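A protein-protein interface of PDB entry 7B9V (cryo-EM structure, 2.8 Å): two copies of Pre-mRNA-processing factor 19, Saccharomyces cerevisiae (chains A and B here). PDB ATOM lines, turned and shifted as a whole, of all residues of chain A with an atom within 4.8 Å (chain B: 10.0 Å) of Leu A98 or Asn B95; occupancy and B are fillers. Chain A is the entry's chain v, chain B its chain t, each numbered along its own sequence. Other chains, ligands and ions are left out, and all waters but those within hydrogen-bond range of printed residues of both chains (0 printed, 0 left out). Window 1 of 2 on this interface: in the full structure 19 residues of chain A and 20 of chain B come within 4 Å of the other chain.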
ATOM      1  N   ILE A  91     -13.614   9.831  20.363  1.00  0.00           N
ATOM      2  CA  ILE A  91     -12.470  10.423  21.080  1.00  0.00           C
ATOM      3  C   ILE A  91     -12.237  11.898  20.706  1.00  0.00           C
ATOM      4  O   ILE A  91     -11.738  12.671  21.527  1.00  0.00           O
ATOM      5  CB  ILE A  91     -11.166   9.586  20.986  1.00  0.00           C
ATOM      6  CG1 ILE A  91     -10.563   9.504  19.589  1.00  0.00           C
ATOM      7  CG2 ILE A  91     -11.366   8.185  21.582  1.00  0.00           C
ATOM      8  CD1 ILE A  91      -9.116   9.028  19.570  1.00  0.00           C
ATOM      9  N   GLU A  94     -14.984  13.636  22.630  1.00  0.00           N
ATOM     10  CA  GLU A  94     -14.488  13.400  23.987  1.00  0.00           C
ATOM     11  C   GLU A  94     -13.335  14.333  24.380  1.00  0.00           C
ATOM     12  O   GLU A  94     -13.285  14.803  25.521  1.00  0.00           O
ATOM     13  CB  GLU A  94     -14.088  11.927  24.162  1.00  0.00           C
ATOM     14  CG  GLU A  94     -13.722  11.530  25.590  1.00  0.00           C
ATOM     15  N   ASN A  95     -12.400  14.618  23.457  1.00  0.00           N
ATOM     16  CA  ASN A  95     -11.319  15.596  23.718  1.00  0.00           C
ATOM     17  C   ASN A  95     -11.874  17.012  23.867  1.00  0.00           C
ATOM     18  O   ASN A  95     -11.440  17.753  24.764  1.00  0.00           O
ATOM     19  CB  ASN A  95     -10.164  15.562  22.680  1.00  0.00           C
ATOM     20  CG  ASN A  95     -10.512  16.138  21.342  1.00  0.00           C
ATOM     21  N   PHE A  96     -12.856  17.385  23.037  1.00  0.00           N
ATOM     22  CA  PHE A  96     -13.510  18.695  23.169  1.00  0.00           C
ATOM     23  C   PHE A  96     -14.294  18.858  24.488  1.00  0.00           C
ATOM     24  O   PHE A  96     -14.151  19.883  25.178  1.00  0.00           O
ATOM     25  CB  PHE A  96     -14.411  18.980  21.941  1.00  0.00           C
ATOM     26  CG  PHE A  96     -15.111  20.350  21.968  1.00  0.00           C
ATOM     27  CD1 PHE A  96     -16.324  20.585  22.650  1.00  0.00           C
ATOM     28  CD2 PHE A  96     -14.472  21.417  21.377  1.00  0.00           C
ATOM     29  CE1 PHE A  96     -16.890  21.833  22.677  1.00  0.00           C
ATOM     30  CE2 PHE A  96     -15.040  22.675  21.407  1.00  0.00           C
ATOM     31  CZ  PHE A  96     -16.244  22.883  22.056  1.00  0.00           C
ATOM     32  N   LYS A  97     -15.059  17.847  24.891  1.00  0.00           N
ATOM     33  CA  LYS A  97     -15.768  17.863  26.185  1.00  0.00           C
ATOM     34  C   LYS A  97     -14.791  17.778  27.366  1.00  0.00           C
ATOM     35  O   LYS A  97     -15.087  18.331  28.428  1.00  0.00           O
ATOM     36  CB  LYS A  97     -16.887  16.807  26.270  1.00  0.00           C
ATOM     37  CG  LYS A  97     -16.514  15.345  26.322  1.00  0.00           C
ATOM     38  N   LEU A  98     -13.729  16.978  27.271  1.00  0.00           N
ATOM     39  CA  LEU A  98     -12.678  16.926  28.296  1.00  0.00           C
ATOM     40  C   LEU A  98     -12.069  18.317  28.528  1.00  0.00           C
ATOM     41  O   LEU A  98     -11.853  18.716  29.677  1.00  0.00           O
ATOM     42  CB  LEU A  98     -11.602  15.922  27.907  1.00  0.00           C
ATOM     43  CG  LEU A  98     -10.356  15.876  28.780  1.00  0.00           C
ATOM     44  CD1 LEU A  98     -10.722  15.492  30.187  1.00  0.00           C
ATOM     45  CD2 LEU A  98      -9.517  14.810  28.206  1.00  0.00           C
ATOM     46  N   ARG A  99     -11.732  19.030  27.453  1.00  0.00           N
ATOM     47  CA  ARG A  99     -11.306  20.438  27.548  1.00  0.00           C
ATOM     48  C   ARG A  99     -12.367  21.332  28.241  1.00  0.00           C
ATOM     49  O   ARG A  99     -12.026  22.118  29.135  1.00  0.00           O
ATOM     50  CB  ARG A  99     -10.954  20.970  26.150  1.00  0.00           C
ATOM     51  CG  ARG A  99     -10.359  22.381  26.120  1.00  0.00           C
ATOM     52  CD  ARG A  99      -9.800  22.754  24.744  1.00  0.00           C
ATOM     53  NE  ARG A  99     -10.850  22.918  23.736  1.00  0.00           N
ATOM     54  CZ  ARG A  99     -10.627  23.016  22.433  1.00  0.00           C
ATOM     55  NH1 ARG A  99      -9.398  22.947  21.934  1.00  0.00           N
ATOM     56  NH2 ARG A  99     -11.659  23.181  21.610  1.00  0.00           N
ATOM     57  N   SER A 100     -13.651  21.197  27.888  1.00  0.00           N
ATOM     58  CA  SER A 100     -14.733  22.023  28.482  1.00  0.00           C
ATOM     59  C   SER A 100     -15.070  21.678  29.961  1.00  0.00           C
ATOM     60  O   SER A 100     -15.244  22.598  30.799  1.00  0.00           O
ATOM     61  CB  SER A 100     -15.991  21.894  27.614  1.00  0.00           C
ATOM     62  OG  SER A 100     -15.720  22.229  26.262  1.00  0.00           O
ATOM     63  N   THR A 101     -14.940  20.412  30.367  1.00  0.00           N
ATOM     64  CA  THR A 101     -15.070  20.060  31.794  1.00  0.00           C
ATOM     65  C   THR A 101     -13.807  20.437  32.581  1.00  0.00           C
ATOM     66  O   THR A 101     -13.914  20.826  33.761  1.00  0.00           O
ATOM     67  CB  THR A 101     -15.480  18.579  31.991  1.00  0.00           C
ATOM     68  OG1 THR A 101     -15.788  18.353  33.371  1.00  0.00           O
ATOM     69  CG2 THR A 101     -14.419  17.550  31.535  1.00  0.00           C
ATOM     70  N   LEU A 102     -12.611  20.265  31.987  1.00  0.00           N
ATOM     71  CA  LEU A 102     -11.372  20.798  32.566  1.00  0.00           C
ATOM     72  C   LEU A 102     -11.437  22.312  32.801  1.00  0.00           C
ATOM     73  O   LEU A 102     -10.851  22.815  33.773  1.00  0.00           O
ATOM     74  CB  LEU A 102     -10.158  20.457  31.683  1.00  0.00           C
ATOM     75  CG  LEU A 102      -8.741  20.955  32.045  1.00  0.00           C
ATOM     76  CD1 LEU A 102      -7.776  19.967  31.620  1.00  0.00           C
ATOM     77  CD2 LEU A 102      -8.309  22.229  31.305  1.00  0.00           C
ATOM     78  N   GLU B  87      -1.435  10.676  14.245  1.00  0.00           N
ATOM     79  CA  GLU B  87      -2.547  11.570  14.558  1.00  0.00           C
ATOM     80  C   GLU B  87      -3.267  11.092  15.802  1.00  0.00           C
ATOM     81  O   GLU B  87      -3.540  11.897  16.683  1.00  0.00           O
ATOM     82  CB  GLU B  87      -3.532  11.689  13.386  1.00  0.00           C
ATOM     83  CG  GLU B  87      -3.017  12.408  12.156  1.00  0.00           C
ATOM     84  CD  GLU B  87      -3.750  11.989  10.898  1.00  0.00           C
ATOM     85  OE1 GLU B  87      -4.986  11.796  10.939  1.00  0.00           O
ATOM     86  OE2 GLU B  87      -3.070  11.828   9.861  1.00  0.00           O
ATOM     87  N   TRP B  88      -3.558   9.794  15.896  1.00  0.00           N
ATOM     88  CA  TRP B  88      -4.071   9.182  17.130  1.00  0.00           C
ATOM     89  C   TRP B  88      -3.094   9.378  18.291  1.00  0.00           C
ATOM     90  O   TRP B  88      -3.546   9.627  19.404  1.00  0.00           O
ATOM     91  CB  TRP B  88      -4.372   7.694  16.915  1.00  0.00           C
ATOM     92  CG  TRP B  88      -4.838   6.954  18.164  1.00  0.00           C
ATOM     93  CD1 TRP B  88      -6.117   6.897  18.634  1.00  0.00           C
ATOM     94  CD2 TRP B  88      -4.046   6.151  19.059  1.00  0.00           C
ATOM     95  NE1 TRP B  88      -6.180   6.130  19.767  1.00  0.00           N
ATOM     96  CE2 TRP B  88      -4.928   5.657  20.047  1.00  0.00           C
ATOM     97  CE3 TRP B  88      -2.699   5.813  19.126  1.00  0.00           C
ATOM     98  CZ2 TRP B  88      -4.491   4.847  21.091  1.00  0.00           C
ATOM     99  CZ3 TRP B  88      -2.269   5.006  20.156  1.00  0.00           C
ATOM    100  CH2 TRP B  88      -3.163   4.533  21.122  1.00  0.00           C
ATOM    101  N   ASP B  89      -1.781   9.210  18.073  1.00  0.00           N
ATOM    102  CA  ASP B  89      -0.768   9.551  19.090  1.00  0.00           C
ATOM    103  C   ASP B  89      -0.912  10.998  19.574  1.00  0.00           C
ATOM    104  O   ASP B  89      -0.925  11.255  20.783  1.00  0.00           O
ATOM    105  CB  ASP B  89       0.689   9.356  18.622  1.00  0.00           C
ATOM    106  CG  ASP B  89       1.057   7.926  18.290  1.00  0.00           C
ATOM    107  OD1 ASP B  89       0.486   6.992  18.886  1.00  0.00           O
ATOM    108  OD2 ASP B  89       1.986   7.742  17.470  1.00  0.00           O
ATOM    109  N   ALA B  90      -0.953  11.954  18.643  1.00  0.00           N
ATOM    110  CA  ALA B  90      -1.111  13.382  18.957  1.00  0.00           C
ATOM    111  C   ALA B  90      -2.445  13.689  19.641  1.00  0.00           C
ATOM    112  O   ALA B  90      -2.490  14.516  20.560  1.00  0.00           O
ATOM    113  CB  ALA B  90      -0.970  14.215  17.682  1.00  0.00           C
ATOM    114  N   ILE B  91      -3.533  13.047  19.198  1.00  0.00           N
ATOM    115  CA  ILE B  91      -4.844  13.154  19.857  1.00  0.00           C
ATOM    116  C   ILE B  91      -4.772  12.649  21.294  1.00  0.00           C
ATOM    117  O   ILE B  91      -5.094  13.389  22.217  1.00  0.00           O
ATOM    118  CB  ILE B  91      -5.950  12.420  19.064  1.00  0.00           C
ATOM    119  CG1 ILE B  91      -6.264  13.106  17.739  1.00  0.00           C
ATOM    120  CG2 ILE B  91      -7.225  12.313  19.884  1.00  0.00           C
ATOM    121  CD1 ILE B  91      -6.932  12.179  16.741  1.00  0.00           C
ATOM    122  N   MET B  92      -4.263  11.436  21.505  1.00  0.00           N
ATOM    123  CA  MET B  92      -4.152  10.812  22.829  1.00  0.00           C
ATOM    124  C   MET B  92      -3.172  11.556  23.743  1.00  0.00           C
ATOM    125  O   MET B  92      -3.408  11.630  24.949  1.00  0.00           O
ATOM    126  CB  MET B  92      -3.799   9.328  22.734  1.00  0.00           C
ATOM    127  CG  MET B  92      -4.897   8.532  22.043  1.00  0.00           C
ATOM    128  SD  MET B  92      -6.593   8.738  22.588  1.00  0.00           S
ATOM    129  CE  MET B  92      -6.568   7.752  24.057  1.00  0.00           C
ATOM    130  N   LEU B  93      -2.110  12.154  23.184  1.00  0.00           N
ATOM    131  CA  LEU B  93      -1.222  13.063  23.928  1.00  0.00           C
ATOM    132  C   LEU B  93      -1.905  14.380  24.306  1.00  0.00           C
ATOM    133  O   LEU B  93      -1.711  14.869  25.423  1.00  0.00           O
ATOM    134  CB  LEU B  93       0.067  13.330  23.141  1.00  0.00           C
ATOM    135  CG  LEU B  93       1.096  14.325  23.716  1.00  0.00           C
ATOM    136  CD1 LEU B  93       2.488  13.789  23.545  1.00  0.00           C
ATOM    137  CD2 LEU B  93       1.050  15.693  23.015  1.00  0.00           C
ATOM    138  N   GLU B  94      -2.700  14.964  23.413  1.00  0.00           N
ATOM    139  CA  GLU B  94      -3.503  16.151  23.736  1.00  0.00           C
ATOM    140  C   GLU B  94      -4.547  15.832  24.810  1.00  0.00           C
ATOM    141  O   GLU B  94      -4.690  16.565  25.798  1.00  0.00           O
ATOM    142  CB  GLU B  94      -4.174  16.709  22.476  1.00  0.00           C
ATOM    143  CG  GLU B  94      -5.161  17.842  22.740  1.00  0.00           C
ATOM    144  N   ASN B  95      -5.335  14.786  24.592  1.00  0.00           N
ATOM    145  CA  ASN B  95      -6.350  14.344  25.554  1.00  0.00           C
ATOM    146  C   ASN B  95      -5.738  13.908  26.889  1.00  0.00           C
ATOM    147  O   ASN B  95      -6.332  14.132  27.941  1.00  0.00           O
ATOM    148  CB  ASN B  95      -7.127  13.139  25.011  1.00  0.00           C
ATOM    149  CG  ASN B  95      -7.750  13.385  23.674  1.00  0.00           C
ATOM    150  N   PHE B  96      -4.553  13.296  26.890  1.00  0.00           N
ATOM    151  CA  PHE B  96      -3.912  13.024  28.177  1.00  0.00           C
ATOM    152  C   PHE B  96      -3.146  14.211  28.798  1.00  0.00           C
ATOM    153  O   PHE B  96      -3.025  14.254  30.015  1.00  0.00           O
ATOM    154  CB  PHE B  96      -3.070  11.752  28.148  1.00  0.00           C
ATOM    155  CG  PHE B  96      -2.691  11.322  29.519  1.00  0.00           C
ATOM    156  CD1 PHE B  96      -3.658  10.719  30.302  1.00  0.00           C
ATOM    157  CD2 PHE B  96      -1.428  11.566  30.050  1.00  0.00           C
ATOM    158  CE1 PHE B  96      -3.391  10.378  31.593  1.00  0.00           C
ATOM    159  CE2 PHE B  96      -1.152  11.210  31.345  1.00  0.00           C
ATOM    160  CZ  PHE B  96      -2.141  10.603  32.105  1.00  0.00           C
ATOM    161  N   LYS B  97      -2.693  15.211  28.044  1.00  0.00           N
ATOM    162  CA  LYS B  97      -2.179  16.435  28.691  1.00  0.00           C
ATOM    163  C   LYS B  97      -3.348  17.166  29.355  1.00  0.00           C
ATOM    164  O   LYS B  97      -3.226  17.639  30.492  1.00  0.00           O
ATOM    165  CB  LYS B  97      -1.353  17.336  27.747  1.00  0.00           C
ATOM    166  CG  LYS B  97      -2.041  18.177  26.671  1.00  0.00           C
ATOM    167  N   LEU B  98      -4.515  17.113  28.718  1.00  0.00           N
ATOM    168  CA  LEU B  98      -5.788  17.459  29.361  1.00  0.00           C
ATOM    169  C   LEU B  98      -6.111  16.558  30.579  1.00  0.00           C
ATOM    170  O   LEU B  98      -6.441  17.079  31.638  1.00  0.00           O
ATOM    171  CB  LEU B  98      -6.915  17.461  28.329  1.00  0.00           C
ATOM    172  CG  LEU B  98      -6.856  18.559  27.258  1.00  0.00           C
ATOM    173  CD1 LEU B  98      -7.889  18.316  26.167  1.00  0.00           C
ATOM    174  CD2 LEU B  98      -7.068  19.936  27.868  1.00  0.00           C
ATOM    175  N   ARG B  99      -6.064  15.226  30.468  1.00  0.00           N
ATOM    176  CA  ARG B  99      -6.333  14.326  31.622  1.00  0.00           C
ATOM    177  C   ARG B  99      -5.318  14.470  32.771  1.00  0.00           C
ATOM    178  O   ARG B  99      -5.703  14.407  33.940  1.00  0.00           O
ATOM    179  CB  ARG B  99      -6.421  12.851  31.212  1.00  0.00           C
ATOM    180  CG  ARG B  99      -7.686  12.453  30.464  1.00  0.00           C
ATOM    181  CD  ARG B  99      -7.817  10.923  30.327  1.00  0.00           C
ATOM    182  NE  ARG B  99      -7.126  10.355  29.169  1.00  0.00           N
ATOM    183  CZ  ARG B  99      -7.585  10.386  27.923  1.00  0.00           C
ATOM    184  NH1 ARG B  99      -8.733  10.980  27.621  1.00  0.00           N
ATOM    185  NH2 ARG B  99      -6.874   9.810  26.957  1.00  0.00           N
ATOM    186  N   SER B 100      -4.029  14.539  32.472  1.00  0.00           N
ATOM    187  CA  SER B 100      -2.962  14.769  33.457  1.00  0.00           C
ATOM    188  C   SER B 100      -3.128  16.122  34.154  1.00  0.00           C
ATOM    189  O   SER B 100      -3.000  16.209  35.387  1.00  0.00           O
ATOM    190  CB  SER B 100      -1.581  14.677  32.797  1.00  0.00           C
ATOM    191  OG  SER B 100      -0.555  14.815  33.769  1.00  0.00           O
ATOM    192  N   THR B 101      -3.498  17.164  33.398  1.00  0.00           N
ATOM    193  CA  THR B 101      -3.913  18.438  33.994  1.00  0.00           C
ATOM    194  C   THR B 101      -5.191  18.286  34.833  1.00  0.00           C
ATOM    195  O   THR B 101      -5.232  18.803  35.943  1.00  0.00           O
ATOM    196  CB  THR B 101      -4.080  19.504  32.898  1.00  0.00           C
ATOM    197  OG1 THR B 101      -2.820  19.755  32.259  1.00  0.00           O
ATOM    198  CG2 THR B 101      -4.581  20.827  33.498  1.00  0.00           C
ATOM    199  N   LEU B 102      -6.223  17.584  34.341  1.00  0.00           N
ATOM    200  CA  LEU B 102      -7.493  17.397  35.069  1.00  0.00           C
ATOM    201  C   LEU B 102      -7.290  16.607  36.370  1.00  0.00           C
ATOM    202  O   LEU B 102      -7.868  16.961  37.398  1.00  0.00           O
ATOM    203  CB  LEU B 102      -8.594  16.760  34.193  1.00  0.00           C
ATOM    204  CG  LEU B 102     -10.055  16.915  34.713  1.00  0.00           C
ATOM    205  CD1 LEU B 102     -11.033  16.864  33.591  1.00  0.00           C
ATOM    206  CD2 LEU B 102     -10.569  15.820  35.689  1.00  0.00           C
ATOM    207  N   ASP B 103      -6.505  15.537  36.340  1.00  0.00           N
ATOM    208  CA  ASP B 103      -6.199  14.729  37.525  1.00  0.00           C
ATOM    209  C   ASP B 103      -5.382  15.531  38.536  1.00  0.00           C
ATOM    210  O   ASP B 103      -5.717  15.553  39.725  1.00  0.00           O
ATOM    211  CB  ASP B 103      -5.446  13.446  37.145  1.00  0.00           C
ATOM    212  CG  ASP B 103      -5.359  12.465  38.300  1.00  0.00           C
ATOM    213  N   LEU B 105      -5.185  18.936  38.681  1.00  0.00           N
ATOM    214  CA  LEU B 105      -6.040  20.058  39.127  1.00  0.00           C
ATOM    215  C   LEU B 105      -7.176  19.613  40.054  1.00  0.00           C
ATOM    216  O   LEU B 105      -7.560  20.369  40.941  1.00  0.00           O
ATOM    217  CB  LEU B 105      -6.625  20.885  37.987  1.00  0.00           C
ATOM    218  CG  LEU B 105      -7.742  20.496  37.050  1.00  0.00           C
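Of chain B, only Asn B95, Leu B98, Arg B99 and Leu B102 come within 4 Å of Leu A98. Asn B95 touches just these residues of chain A: Asn A95 and Leu A98. No residue of chain B comes within 4 Å of Glu A94. No residue of chain B comes within 4 Å of Lys A97. No residue of chain B comes within 4 Å of Ser A100. No residue of chain B comes within 4 Å of Thr A101. Of chain B, only Leu B98 (3.2 Å), Thr B101 (3.8 Å) and Leu B102 (3.9 Å) come within 4 Å of Leu A102. Of the printed residues of chain A, Arg B99 touches Leu A98. Of the printed residues of chain A, Leu B102 touches Leu A98 and Leu A102. Glu B87 touches none of the printed residues of chain A. The nearest residue of chain B that does not touch Leu A98 is Phe B96 (5.4 Å). The nearest printed residue of chain A that does not touch Thr B101 is Leu A98 (7.7 Å).
Asn A95 touches Leu B98, and with the chains exchanged Leu A98 touches Asn B95. Leu A98 touches Leu B102, and with the chains exchanged Leu A102 touches Leu B98. Leu A102 touches Thr B101, but with the chains exchanged Thr A101 does not touch Leu B102 (4.02 Å). Leu A102 touches its own counterpart, Leu B102. Of the 12 pairs that touch across the chains among the printed residues, 8 have their exchanged pair printed and touching as well.
Ile A91 touches Trp B88 (CD1 to CD1, 3.8 Å). Met B92 touches Ile A91 (SD to CD1, 3.9 Å). CB of Asn A95 touches CG of Asn B95 (3.4 Å). CD1 of Leu B98 touches O of Asn A95, at 3.9 Å. Leu A98 touches Asn B95. Leu A98 touches Leu B98 (CD2 to CB, 3.7 Å). CD1 of Leu A98 touches CD1 of Leu B102 (3.7 Å). CD1 of Leu A102 touches O of Leu B98, 3.2 Å away. CD1 of Leu A102 touches CG2 of Thr B101, at 3.8 Å. Leu B102 touches Leu A102.
Printed residues of chain A that touch a printed residue of chain B: Ile A91, Asn A95, Leu A98 and Leu A102. Of the 18 printed residues of chain B, 8 touch a printed residue of chain A. Hydrophobic or aromatic side chains of chain B that line the printed part of chain A: Trp B88, Ile B91, Met B92, Leu B98 and Leu B102. Among the printed residues, 12 pairs touch across the chains.
The backbone carbonyl oxygen (O) of Lys B97 sits at hydrogen-bond distance from the side-chain hydroxyl (OG1) of Thr B101 (2.8 Å).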
